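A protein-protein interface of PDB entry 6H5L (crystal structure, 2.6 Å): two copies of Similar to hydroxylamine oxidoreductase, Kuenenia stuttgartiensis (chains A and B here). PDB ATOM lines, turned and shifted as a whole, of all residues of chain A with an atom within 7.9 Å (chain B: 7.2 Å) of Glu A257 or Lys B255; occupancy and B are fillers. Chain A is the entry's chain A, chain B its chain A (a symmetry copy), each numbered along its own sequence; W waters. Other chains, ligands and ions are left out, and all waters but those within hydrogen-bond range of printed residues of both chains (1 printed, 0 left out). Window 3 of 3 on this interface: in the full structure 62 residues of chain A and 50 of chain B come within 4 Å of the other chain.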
ATOM      1  N   VAL A 221      -2.187  17.107   6.189  1.00  0.00           N
ATOM      2  CA  VAL A 221      -2.899  15.950   5.652  1.00  0.00           C
ATOM      3  C   VAL A 221      -3.685  16.344   4.410  1.00  0.00           C
ATOM      4  O   VAL A 221      -3.684  15.630   3.401  1.00  0.00           O
ATOM      5  CB  VAL A 221      -3.812  15.339   6.731  1.00  0.00           C
ATOM      6  CG1 VAL A 221      -4.719  14.277   6.126  1.00  0.00           C
ATOM      7  CG2 VAL A 221      -2.979  14.754   7.862  1.00  0.00           C
ATOM      8  N   GLU A 222      -4.359  17.495   4.457  1.00  0.00           N
ATOM      9  CA  GLU A 222      -5.138  17.933   3.303  1.00  0.00           C
ATOM     10  C   GLU A 222      -4.234  18.380   2.162  1.00  0.00           C
ATOM     11  O   GLU A 222      -4.562  18.179   0.987  1.00  0.00           O
ATOM     12  CB  GLU A 222      -6.091  19.055   3.705  1.00  0.00           C
ATOM     13  CG  GLU A 222      -7.035  19.481   2.598  1.00  0.00           C
ATOM     14  CD  GLU A 222      -7.661  20.829   2.864  1.00  0.00           C
ATOM     15  OE1 GLU A 222      -8.221  21.028   3.963  1.00  0.00           O
ATOM     16  OE2 GLU A 222      -7.577  21.698   1.974  1.00  0.00           O
ATOM     17  N   GLN A 225      -3.098  15.286   0.050  1.00  0.00           N
ATOM     18  CA  GLN A 225      -3.939  14.440  -0.787  1.00  0.00           C
ATOM     19  C   GLN A 225      -4.144  15.081  -2.157  1.00  0.00           C
ATOM     20  O   GLN A 225      -4.183  16.311  -2.269  1.00  0.00           O
ATOM     21  CB  GLN A 225      -5.284  14.185  -0.117  1.00  0.00           C
ATOM     22  CG  GLN A 225      -5.730  15.262   0.851  1.00  0.00           C
ATOM     23  CD  GLN A 225      -6.773  14.762   1.833  1.00  0.00           C
ATOM     24  OE1 GLN A 225      -6.766  13.593   2.222  1.00  0.00           O
ATOM     25  NE2 GLN A 225      -7.678  15.644   2.236  1.00  0.00           N
ATOM     26  N   PRO A 226      -4.268  14.258  -3.206  1.00  0.00           N
ATOM     27  CA  PRO A 226      -4.321  14.800  -4.575  1.00  0.00           C
ATOM     28  C   PRO A 226      -5.432  15.808  -4.815  1.00  0.00           C
ATOM     29  O   PRO A 226      -5.276  16.690  -5.670  1.00  0.00           O
ATOM     30  CB  PRO A 226      -4.518  13.544  -5.433  1.00  0.00           C
ATOM     31  CG  PRO A 226      -3.917  12.450  -4.638  1.00  0.00           C
ATOM     32  CD  PRO A 226      -4.188  12.788  -3.196  1.00  0.00           C
ATOM     33  N   GLU A 227      -6.548  15.709  -4.089  1.00  0.00           N
ATOM     34  CA  GLU A 227      -7.682  16.594  -4.337  1.00  0.00           C
ATOM     35  C   GLU A 227      -7.362  18.056  -4.053  1.00  0.00           C
ATOM     36  O   GLU A 227      -8.091  18.938  -4.519  1.00  0.00           O
ATOM     37  CB  GLU A 227      -8.890  16.156  -3.505  1.00  0.00           C
ATOM     38  CG  GLU A 227      -9.614  14.914  -4.024  1.00  0.00           C
ATOM     39  CD  GLU A 227      -8.894  13.617  -3.695  1.00  0.00           C
ATOM     40  OE1 GLU A 227      -9.397  12.540  -4.085  1.00  0.00           O
ATOM     41  OE2 GLU A 227      -7.830  13.669  -3.042  1.00  0.00           O
ATOM     42  N   ALA A 228      -6.295  18.337  -3.300  1.00  0.00           N
ATOM     43  CA  ALA A 228      -5.941  19.719  -2.999  1.00  0.00           C
ATOM     44  C   ALA A 228      -5.464  20.483  -4.227  1.00  0.00           C
ATOM     45  O   ALA A 228      -5.502  21.718  -4.226  1.00  0.00           O
ATOM     46  CB  ALA A 228      -4.865  19.761  -1.913  1.00  0.00           C
ATOM     47  N   MET A 230      -6.690  19.791  -7.442  1.00  0.00           N
ATOM     48  CA  MET A 230      -7.581  19.562  -8.573  1.00  0.00           C
ATOM     49  C   MET A 230      -8.531  20.723  -8.843  1.00  0.00           C
ATOM     50  O   MET A 230      -9.127  20.773  -9.924  1.00  0.00           O
ATOM     51  CB  MET A 230      -8.373  18.270  -8.354  1.00  0.00           C
ATOM     52  CG  MET A 230      -7.495  17.087  -7.975  1.00  0.00           C
ATOM     53  SD  MET A 230      -8.282  15.492  -8.268  1.00  0.00           S
ATOM     54  CE  MET A 230      -9.911  15.797  -7.598  1.00  0.00           C
ATOM     55  N   GLY A 250      -4.787   6.763  -9.821  1.00  0.00           N
ATOM     56  CA  GLY A 250      -5.841   7.500  -9.156  1.00  0.00           C
ATOM     57  C   GLY A 250      -7.018   6.642  -8.740  1.00  0.00           C
ATOM     58  O   GLY A 250      -7.608   6.864  -7.677  1.00  0.00           O
ATOM     59  N   LYS A 251      -7.378   5.661  -9.574  1.00  0.00           N
ATOM     60  CA  LYS A 251      -8.472   4.761  -9.223  1.00  0.00           C
ATOM     61  C   LYS A 251      -8.134   3.942  -7.984  1.00  0.00           C
ATOM     62  O   LYS A 251      -8.997   3.707  -7.130  1.00  0.00           O
ATOM     63  CB  LYS A 251      -8.800   3.843 -10.400  1.00  0.00           C
ATOM     64  CG  LYS A 251      -9.591   4.518 -11.507  1.00  0.00           C
ATOM     65  CD  LYS A 251     -10.910   5.047 -10.971  1.00  0.00           C
ATOM     66  CE  LYS A 251     -11.122   6.495 -11.366  1.00  0.00           C
ATOM     67  NZ  LYS A 251     -12.200   7.139 -10.566  1.00  0.00           N
ATOM     68  N   ILE A 252      -6.881   3.502  -7.867  1.00  0.00           N
ATOM     69  CA  ILE A 252      -6.472   2.732  -6.698  1.00  0.00           C
ATOM     70  C   ILE A 252      -6.427   3.621  -5.462  1.00  0.00           C
ATOM     71  O   ILE A 252      -6.804   3.198  -4.363  1.00  0.00           O
ATOM     72  CB  ILE A 252      -5.121   2.044  -6.963  1.00  0.00           C
ATOM     73  CG1 ILE A 252      -5.286   0.938  -8.006  1.00  0.00           C
ATOM     74  CG2 ILE A 252      -4.536   1.493  -5.673  1.00  0.00           C
ATOM     75  CD1 ILE A 252      -3.981   0.306  -8.446  1.00  0.00           C
ATOM     76  N   TYR A 253      -5.977   4.867  -5.619  1.00  0.00           N
ATOM     77  CA  TYR A 253      -5.974   5.794  -4.492  1.00  0.00           C
ATOM     78  C   TYR A 253      -7.391   6.082  -4.015  1.00  0.00           C
ATOM     79  O   TYR A 253      -7.669   6.059  -2.812  1.00  0.00           O
ATOM     80  CB  TYR A 253      -5.260   7.092  -4.870  1.00  0.00           C
ATOM     81  CG  TYR A 253      -5.740   8.296  -4.083  1.00  0.00           C
ATOM     82  CD1 TYR A 253      -5.477   8.414  -2.724  1.00  0.00           C
ATOM     83  CD2 TYR A 253      -6.453   9.314  -4.703  1.00  0.00           C
ATOM     84  CE1 TYR A 253      -5.918   9.510  -2.004  1.00  0.00           C
ATOM     85  CE2 TYR A 253      -6.896  10.413  -3.992  1.00  0.00           C
ATOM     86  CZ  TYR A 253      -6.626  10.506  -2.644  1.00  0.00           C
ATOM     87  OH  TYR A 253      -7.064  11.602  -1.934  1.00  0.00           O
ATOM     88  N   GLU A 254      -8.306   6.356  -4.948  1.00  0.00           N
ATOM     89  CA  GLU A 254      -9.670   6.706  -4.561  1.00  0.00           C
ATOM     90  C   GLU A 254     -10.376   5.552  -3.858  1.00  0.00           C
ATOM     91  O   GLU A 254     -11.225   5.781  -2.988  1.00  0.00           O
ATOM     92  CB  GLU A 254     -10.462   7.155  -5.787  1.00  0.00           C
ATOM     93  CG  GLU A 254     -10.108   8.558  -6.257  1.00  0.00           C
ATOM     94  CD  GLU A 254     -10.292   8.746  -7.750  1.00  0.00           C
ATOM     95  OE1 GLU A 254     -10.939   7.889  -8.388  1.00  0.00           O
ATOM     96  OE2 GLU A 254      -9.778   9.751  -8.287  1.00  0.00           O
ATOM     97  N   LYS A 255     -10.044   4.312  -4.212  1.00  0.00           N
ATOM     98  CA  LYS A 255     -10.685   3.148  -3.616  1.00  0.00           C
ATOM     99  C   LYS A 255      -9.917   2.566  -2.436  1.00  0.00           C
ATOM    100  O   LYS A 255     -10.466   1.723  -1.719  1.00  0.00           O
ATOM    101  CB  LYS A 255     -10.897   2.063  -4.678  1.00  0.00           C
ATOM    102  CG  LYS A 255     -11.868   2.463  -5.780  1.00  0.00           C
ATOM    103  CD  LYS A 255     -13.186   2.974  -5.205  1.00  0.00           C
ATOM    104  CE  LYS A 255     -13.942   1.881  -4.457  1.00  0.00           C
ATOM    105  NZ  LYS A 255     -15.187   2.396  -3.820  1.00  0.00           N
ATOM    106  N   GLU A 256      -8.673   2.991  -2.210  1.00  0.00           N
ATOM    107  CA  GLU A 256      -7.893   2.538  -1.063  1.00  0.00           C
ATOM    108  C   GLU A 256      -7.466   3.693  -0.163  1.00  0.00           C
ATOM    109  O   GLU A 256      -6.568   3.520   0.667  1.00  0.00           O
ATOM    110  CB  GLU A 256      -6.658   1.757  -1.522  1.00  0.00           C
ATOM    111  CG  GLU A 256      -6.957   0.488  -2.300  1.00  0.00           C
ATOM    112  CD  GLU A 256      -5.713  -0.354  -2.529  1.00  0.00           C
ATOM    113  OE1 GLU A 256      -4.754  -0.217  -1.742  1.00  0.00           O
ATOM    114  OE2 GLU A 256      -5.689  -1.147  -3.494  1.00  0.00           O
ATOM    115  N   GLU A 257      -8.090   4.868  -0.311  1.00  0.00           N
ATOM    116  CA  GLU A 257      -7.628   6.056   0.406  1.00  0.00           C
ATOM    117  C   GLU A 257      -7.697   5.889   1.918  1.00  0.00           C
ATOM    118  O   GLU A 257      -6.915   6.515   2.643  1.00  0.00           O
ATOM    119  CB  GLU A 257      -8.439   7.280  -0.023  1.00  0.00           C
ATOM    120  CG  GLU A 257      -9.904   6.990  -0.285  1.00  0.00           C
ATOM    121  CD  GLU A 257     -10.733   8.250  -0.430  1.00  0.00           C
ATOM    122  OE1 GLU A 257     -10.889   8.978   0.573  1.00  0.00           O
ATOM    123  OE2 GLU A 257     -11.224   8.515  -1.549  1.00  0.00           O
ATOM    124  N   GLU A 258      -8.621   5.062   2.417  1.00  0.00           N
ATOM    125  CA  GLU A 258      -8.735   4.874   3.860  1.00  0.00           C
ATOM    126  C   GLU A 258      -7.453   4.313   4.461  1.00  0.00           C
ATOM    127  O   GLU A 258      -7.143   4.590   5.625  1.00  0.00           O
ATOM    128  CB  GLU A 258      -9.914   3.959   4.189  1.00  0.00           C
ATOM    129  CG  GLU A 258     -11.274   4.593   3.956  1.00  0.00           C
ATOM    130  CD  GLU A 258     -12.029   3.954   2.809  1.00  0.00           C
ATOM    131  OE1 GLU A 258     -13.081   3.330   3.064  1.00  0.00           O
ATOM    132  OE2 GLU A 258     -11.566   4.069   1.654  1.00  0.00           O
ATOM    133  N   HIS A 259      -6.692   3.540   3.689  1.00  0.00           N
ATOM    134  CA  HIS A 259      -5.462   2.931   4.173  1.00  0.00           C
ATOM    135  C   HIS A 259      -4.216   3.703   3.753  1.00  0.00           C
ATOM    136  O   HIS A 259      -3.099   3.224   3.973  1.00  0.00           O
ATOM    137  CB  HIS A 259      -5.382   1.478   3.705  1.00  0.00           C
ATOM    138  CG  HIS A 259      -6.460   0.608   4.270  1.00  0.00           C
ATOM    139  ND1 HIS A 259      -7.734   0.561   3.744  1.00  0.00           N
ATOM    140  CD2 HIS A 259      -6.461  -0.235   5.330  1.00  0.00           C
ATOM    141  CE1 HIS A 259      -8.468  -0.280   4.448  1.00  0.00           C
ATOM    142  NE2 HIS A 259      -7.720  -0.777   5.417  1.00  0.00           N
ATOM    143  N   TYR A 260      -4.383   4.879   3.152  1.00  0.00           N
ATOM    144  CA  TYR A 260      -3.268   5.790   2.929  1.00  0.00           C
ATOM    145  C   TYR A 260      -3.016   6.597   4.197  1.00  0.00           C
ATOM    146  O   TYR A 260      -3.955   7.115   4.809  1.00  0.00           O
ATOM    147  CB  TYR A 260      -3.564   6.733   1.763  1.00  0.00           C
ATOM    148  CG  TYR A 260      -3.315   6.157   0.384  1.00  0.00           C
ATOM    149  CD1 TYR A 260      -3.918   4.973  -0.019  1.00  0.00           C
ATOM    150  CD2 TYR A 260      -2.496   6.816  -0.524  1.00  0.00           C
ATOM    151  CE1 TYR A 260      -3.699   4.453  -1.281  1.00  0.00           C
ATOM    152  CE2 TYR A 260      -2.271   6.305  -1.788  1.00  0.00           C
ATOM    153  CZ  TYR A 260      -2.875   5.124  -2.161  1.00  0.00           C
ATOM    154  OH  TYR A 260      -2.653   4.613  -3.419  1.00  0.00           O
ATOM    155  N   ASP A 261      -1.752   6.704   4.595  1.00  0.00           N
ATOM    156  CA  ASP A 261      -1.378   7.443   5.802  1.00  0.00           C
ATOM    157  C   ASP A 261      -0.869   8.813   5.364  1.00  0.00           C
ATOM    158  O   ASP A 261       0.316   8.996   5.082  1.00  0.00           O
ATOM    159  CB  ASP A 261      -0.341   6.676   6.615  1.00  0.00           C
ATOM    160  CG  ASP A 261      -0.125   7.267   7.999  1.00  0.00           C
ATOM    161  OD1 ASP A 261      -0.643   8.373   8.270  1.00  0.00           O
ATOM    162  OD2 ASP A 261       0.559   6.621   8.822  1.00  0.00           O
ATOM    163  N   PHE A 262      -1.779   9.784   5.311  1.00  0.00           N
ATOM    164  CA  PHE A 262      -1.424  11.147   4.935  1.00  0.00           C
ATOM    165  C   PHE A 262      -0.874  11.961   6.098  1.00  0.00           C
ATOM    166  O   PHE A 262      -0.516  13.127   5.899  1.00  0.00           O
ATOM    167  CB  PHE A 262      -2.633  11.861   4.327  1.00  0.00           C
ATOM    168  CG  PHE A 262      -3.003  11.366   2.959  1.00  0.00           C
ATOM    169  CD1 PHE A 262      -2.176  11.612   1.873  1.00  0.00           C
ATOM    170  CD2 PHE A 262      -4.177  10.657   2.754  1.00  0.00           C
ATOM    171  CE1 PHE A 262      -2.509  11.158   0.612  1.00  0.00           C
ATOM    172  CE2 PHE A 262      -4.516  10.201   1.496  1.00  0.00           C
ATOM    173  CZ  PHE A 262      -3.681  10.452   0.423  1.00  0.00           C
ATOM    174  N   ASP A 274       2.468   2.536   2.675  1.00  0.00           N
ATOM    175  CA  ASP A 274       1.698   3.718   3.044  1.00  0.00           C
ATOM    176  C   ASP A 274       0.874   4.242   1.871  1.00  0.00           C
ATOM    177  O   ASP A 274      -0.315   4.533   2.029  1.00  0.00           O
ATOM    178  CB  ASP A 274       2.631   4.808   3.578  1.00  0.00           C
ATOM    179  CG  ASP A 274       3.324   4.397   4.860  1.00  0.00           C
ATOM    180  OD1 ASP A 274       2.732   3.603   5.622  1.00  0.00           O
ATOM    181  OD2 ASP A 274       4.459   4.863   5.104  1.00  0.00           O
ATOM    182  N   GLY B 250     -16.450  21.794  -2.552  1.00  0.00           N
ATOM    183  CA  GLY B 250     -16.723  20.409  -2.872  1.00  0.00           C
ATOM    184  C   GLY B 250     -15.558  19.479  -2.601  1.00  0.00           C
ATOM    185  O   GLY B 250     -15.757  18.340  -2.164  1.00  0.00           O
ATOM    186  N   LYS B 251     -14.335  19.947  -2.866  1.00  0.00           N
ATOM    187  CA  LYS B 251     -13.158  19.131  -2.588  1.00  0.00           C
ATOM    188  C   LYS B 251     -13.018  18.857  -1.096  1.00  0.00           C
ATOM    189  O   LYS B 251     -12.646  17.749  -0.691  1.00  0.00           O
ATOM    190  CB  LYS B 251     -11.901  19.812  -3.128  1.00  0.00           C
ATOM    191  CG  LYS B 251     -11.736  19.696  -4.634  1.00  0.00           C
ATOM    192  CD  LYS B 251     -11.668  18.238  -5.052  1.00  0.00           C
ATOM    193  CE  LYS B 251     -12.632  17.946  -6.186  1.00  0.00           C
ATOM    194  NZ  LYS B 251     -12.856  16.486  -6.366  1.00  0.00           N
ATOM    195  N   ILE B 252     -13.315  19.854  -0.263  1.00  0.00           N
ATOM    196  CA  ILE B 252     -13.230  19.664   1.181  1.00  0.00           C
ATOM    197  C   ILE B 252     -14.341  18.739   1.664  1.00  0.00           C
ATOM    198  O   ILE B 252     -14.128  17.904   2.550  1.00  0.00           O
ATOM    199  CB  ILE B 252     -13.263  21.026   1.897  1.00  0.00           C
ATOM    200  CG1 ILE B 252     -11.972  21.800   1.622  1.00  0.00           C
ATOM    201  CG2 ILE B 252     -13.480  20.844   3.390  1.00  0.00           C
ATOM    202  CD1 ILE B 252     -11.977  23.217   2.158  1.00  0.00           C
ATOM    203  N   TYR B 253     -15.536  18.863   1.085  1.00  0.00           N
ATOM    204  CA  TYR B 253     -16.625  17.961   1.450  1.00  0.00           C
ATOM    205  C   TYR B 253     -16.295  16.523   1.072  1.00  0.00           C
ATOM    206  O   TYR B 253     -16.489  15.601   1.871  1.00  0.00           O
ATOM    207  CB  TYR B 253     -17.930  18.404   0.788  1.00  0.00           C
ATOM    208  CG  TYR B 253     -18.905  17.267   0.555  1.00  0.00           C
ATOM    209  CD1 TYR B 253     -19.529  16.629   1.620  1.00  0.00           C
ATOM    210  CD2 TYR B 253     -19.201  16.835  -0.731  1.00  0.00           C
ATOM    211  CE1 TYR B 253     -20.415  15.588   1.408  1.00  0.00           C
ATOM    212  CE2 TYR B 253     -20.087  15.797  -0.952  1.00  0.00           C
ATOM    213  CZ  TYR B 253     -20.691  15.177   0.121  1.00  0.00           C
ATOM    214  OH  TYR B 253     -21.575  14.145  -0.097  1.00  0.00           O
ATOM    215  N   GLU B 254     -15.792  16.311  -0.146  1.00  0.00           N
ATOM    216  CA  GLU B 254     -15.512  14.952  -0.601  1.00  0.00           C
ATOM    217  C   GLU B 254     -14.423  14.285   0.233  1.00  0.00           C
ATOM    218  O   GLU B 254     -14.442  13.062   0.415  1.00  0.00           O
ATOM    219  CB  GLU B 254     -15.127  14.964  -2.079  1.00  0.00           C
ATOM    220  CG  GLU B 254     -16.313  15.161  -3.012  1.00  0.00           C
ATOM    221  CD  GLU B 254     -15.940  15.862  -4.303  1.00  0.00           C
ATOM    222  OE1 GLU B 254     -14.731  15.963  -4.604  1.00  0.00           O
ATOM    223  OE2 GLU B 254     -16.859  16.320  -5.014  1.00  0.00           O
ATOM    224  N   LYS B 255     -13.472  15.062   0.748  1.00  0.00           N
ATOM    225  CA  LYS B 255     -12.376  14.510   1.533  1.00  0.00           C
ATOM    226  C   LYS B 255     -12.627  14.540   3.035  1.00  0.00           C
ATOM    227  O   LYS B 255     -11.874  13.907   3.783  1.00  0.00           O
ATOM    228  CB  LYS B 255     -11.074  15.254   1.213  1.00  0.00           C
ATOM    229  CG  LYS B 255     -10.597  15.068  -0.221  1.00  0.00           C
ATOM    230  CD  LYS B 255     -10.527  13.591  -0.599  1.00  0.00           C
ATOM    231  CE  LYS B 255      -9.477  12.844   0.216  1.00  0.00           C
ATOM    232  NZ  LYS B 255      -9.465  11.385  -0.089  1.00  0.00           N
ATOM    233  N   GLU B 256     -13.659  15.248   3.497  1.00  0.00           N
ATOM    234  CA  GLU B 256     -14.010  15.275   4.913  1.00  0.00           C
ATOM    235  C   GLU B 256     -15.429  14.775   5.164  1.00  0.00           C
ATOM    236  O   GLU B 256     -15.976  15.009   6.247  1.00  0.00           O
ATOM    237  CB  GLU B 256     -13.853  16.688   5.485  1.00  0.00           C
ATOM    238  CG  GLU B 256     -12.439  17.242   5.437  1.00  0.00           C
ATOM    239  CD  GLU B 256     -12.303  18.539   6.216  1.00  0.00           C
ATOM    240  OE1 GLU B 256     -13.121  18.768   7.130  1.00  0.00           O
ATOM    241  OE2 GLU B 256     -11.386  19.331   5.914  1.00  0.00           O
ATOM    242  N   GLU B 257     -16.036  14.090   4.187  1.00  0.00           N
ATOM    243  CA  GLU B 257     -17.446  13.718   4.299  1.00  0.00           C
ATOM    244  C   GLU B 257     -17.716  12.807   5.489  1.00  0.00           C
ATOM    245  O   GLU B 257     -18.829  12.815   6.030  1.00  0.00           O
ATOM    246  CB  GLU B 257     -17.918  13.046   3.008  1.00  0.00           C
ATOM    247  CG  GLU B 257     -16.876  12.156   2.357  1.00  0.00           C
ATOM    248  CD  GLU B 257     -17.450  11.293   1.252  1.00  0.00           C
ATOM    249  OE1 GLU B 257     -18.262  10.395   1.562  1.00  0.00           O
ATOM    250  OE2 GLU B 257     -17.097  11.519   0.075  1.00  0.00           O
ATOM    251  N   GLU B 258     -16.727  12.013   5.909  1.00  0.00           N
ATOM    252  CA  GLU B 258     -16.939  11.115   7.040  1.00  0.00           C
ATOM    253  C   GLU B 258     -17.292  11.877   8.311  1.00  0.00           C
ATOM    254  O   GLU B 258     -18.012  11.351   9.167  1.00  0.00           O
ATOM    255  CB  GLU B 258     -15.700  10.249   7.274  1.00  0.00           C
ATOM    256  CG  GLU B 258     -15.475   9.190   6.210  1.00  0.00           C
ATOM    257  CD  GLU B 258     -14.242   9.457   5.370  1.00  0.00           C
ATOM    258  OE1 GLU B 258     -13.283   8.660   5.451  1.00  0.00           O
ATOM    259  OE2 GLU B 258     -14.229  10.469   4.637  1.00  0.00           O
ATOM    260  N   HIS B 259     -16.813  13.111   8.448  1.00  0.00           N
ATOM    261  CA  HIS B 259     -17.069  13.914   9.633  1.00  0.00           C
ATOM    262  C   HIS B 259     -18.196  14.922   9.433  1.00  0.00           C
ATOM    263  O   HIS B 259     -18.425  15.764  10.308  1.00  0.00           O
ATOM    264  CB  HIS B 259     -15.785  14.620  10.070  1.00  0.00           C
ATOM    265  CG  HIS B 259     -14.703  13.681  10.499  1.00  0.00           C
ATOM    266  ND1 HIS B 259     -13.878  13.033   9.604  1.00  0.00           N
ATOM    267  CD2 HIS B 259     -14.323  13.261  11.729  1.00  0.00           C
ATOM    268  CE1 HIS B 259     -13.031  12.265  10.264  1.00  0.00           C
ATOM    269  NE2 HIS B 259     -13.280  12.384  11.555  1.00  0.00           N
ATOM    270  N   TYR B 260     -18.899  14.856   8.305  1.00  0.00           N
ATOM    271  CA  TYR B 260     -20.133  15.610   8.125  1.00  0.00           C
ATOM    272  C   TYR B 260     -21.287  14.845   8.761  1.00  0.00           C
ATOM    273  O   TYR B 260     -21.422  13.634   8.563  1.00  0.00           O
ATOM    274  CB  TYR B 260     -20.415  15.841   6.641  1.00  0.00           C
ATOM    275  CG  TYR B 260     -19.666  16.998   6.010  1.00  0.00           C
ATOM    276  CD1 TYR B 260     -18.281  17.074   6.074  1.00  0.00           C
ATOM    277  CD2 TYR B 260     -20.347  17.997   5.327  1.00  0.00           C
ATOM    278  CE1 TYR B 260     -17.597  18.124   5.488  1.00  0.00           C
ATOM    279  CE2 TYR B 260     -19.672  19.049   4.739  1.00  0.00           C
ATOM    280  CZ  TYR B 260     -18.298  19.107   4.822  1.00  0.00           C
ATOM    281  OH  TYR B 260     -17.623  20.154   4.237  1.00  0.00           O
HETATM  282  O   HOH W   1      -9.820  10.523  -2.365  1.00  0.00           O
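The side-chain amino group (NZ) of Lys B255 is in hydrogen-bond range of the side-chain hydroxyl (OH) of Tyr A253, at 3.0 Å. The side-chain carboxylate (OE1) of Glu A257 is in salt-bridge range of the side-chain amino group (NZ) of Lys B255, 2.9 Å away.
The side-chain carboxylate (OE2) of Glu A227 sits at hydrogen-bond distance from the side-chain hydroxyl (OH) of Tyr A253, 2.5 Å away. The side-chain carboxylate of Glu B254 is in salt-bridge range of the side-chain amino group of Lys B251, 2.6 Å away.
Lys B255 touches Gln A225 (CE to OE1, 3.5 Å). O of Glu A227 touches CD of Lys B251 (3.7 Å). CD of Glu A227 touches CD of Lys B255, 3.5 Å away. Lys B251 touches Met A230.
Of the printed residues of chain B, Gln A225 touches Lys B255. Of the printed residues of chain B, Met A230 touches Lys B251. Of the printed residues of chain B, Tyr A253 touches Lys B255. Glu A257 touches just one residue of chain B: Lys B255. Of chain A, only Gln A225, Glu A227, Tyr A253 and Glu A257 come within 4 Å of Lys B255. The nearest printed residue of chain B that does not touch Glu A257 is Glu B254 (5.4 Å). The nearest printed residue of chain B that does not touch Gln A225 is Glu B256 (6.0 Å).
Printed residues of chain B that touch a printed residue of chain A: Lys B251 and Lys B255. Along chain B the printed residues that touch a printed residue of chain A span positions 251 to 255. Of the 21 printed residues of chain A, 5 touch a printed residue of chain B. Printed residues of chain A that touch a printed residue of chain B: Gln A225, Glu A227, Met A230, Tyr A253 and Glu A257. Hydrophobic or aromatic side chains of chain A within 4 Å of the printed part of chain B: Met A230 and Tyr A253. Among the printed residues, 6 pairs touch across the chains.
Tyr A253 touches Lys B255, but with the chains exchanged Lys A255 does not touch Tyr B253 (13.9 Å). Glu A257 touches Lys B255, but with the chains exchanged Lys A255 does not touch Glu B257 (10.1 Å). Positions printed for both chains: 250, 251, 252, 253, 254, 255, 256, 257, 258, 259 and 260.
Water W1 lies within hydrogen-bond range of the side-chain amino group of Lys B255 (2.5 Å), the side-chain carboxylate of Glu A257 (2.6 Å), the side-chain carboxylate of Glu A227 (2.7 Å) and the side-chain hydroxyl of Tyr A253 (3.0 Å).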
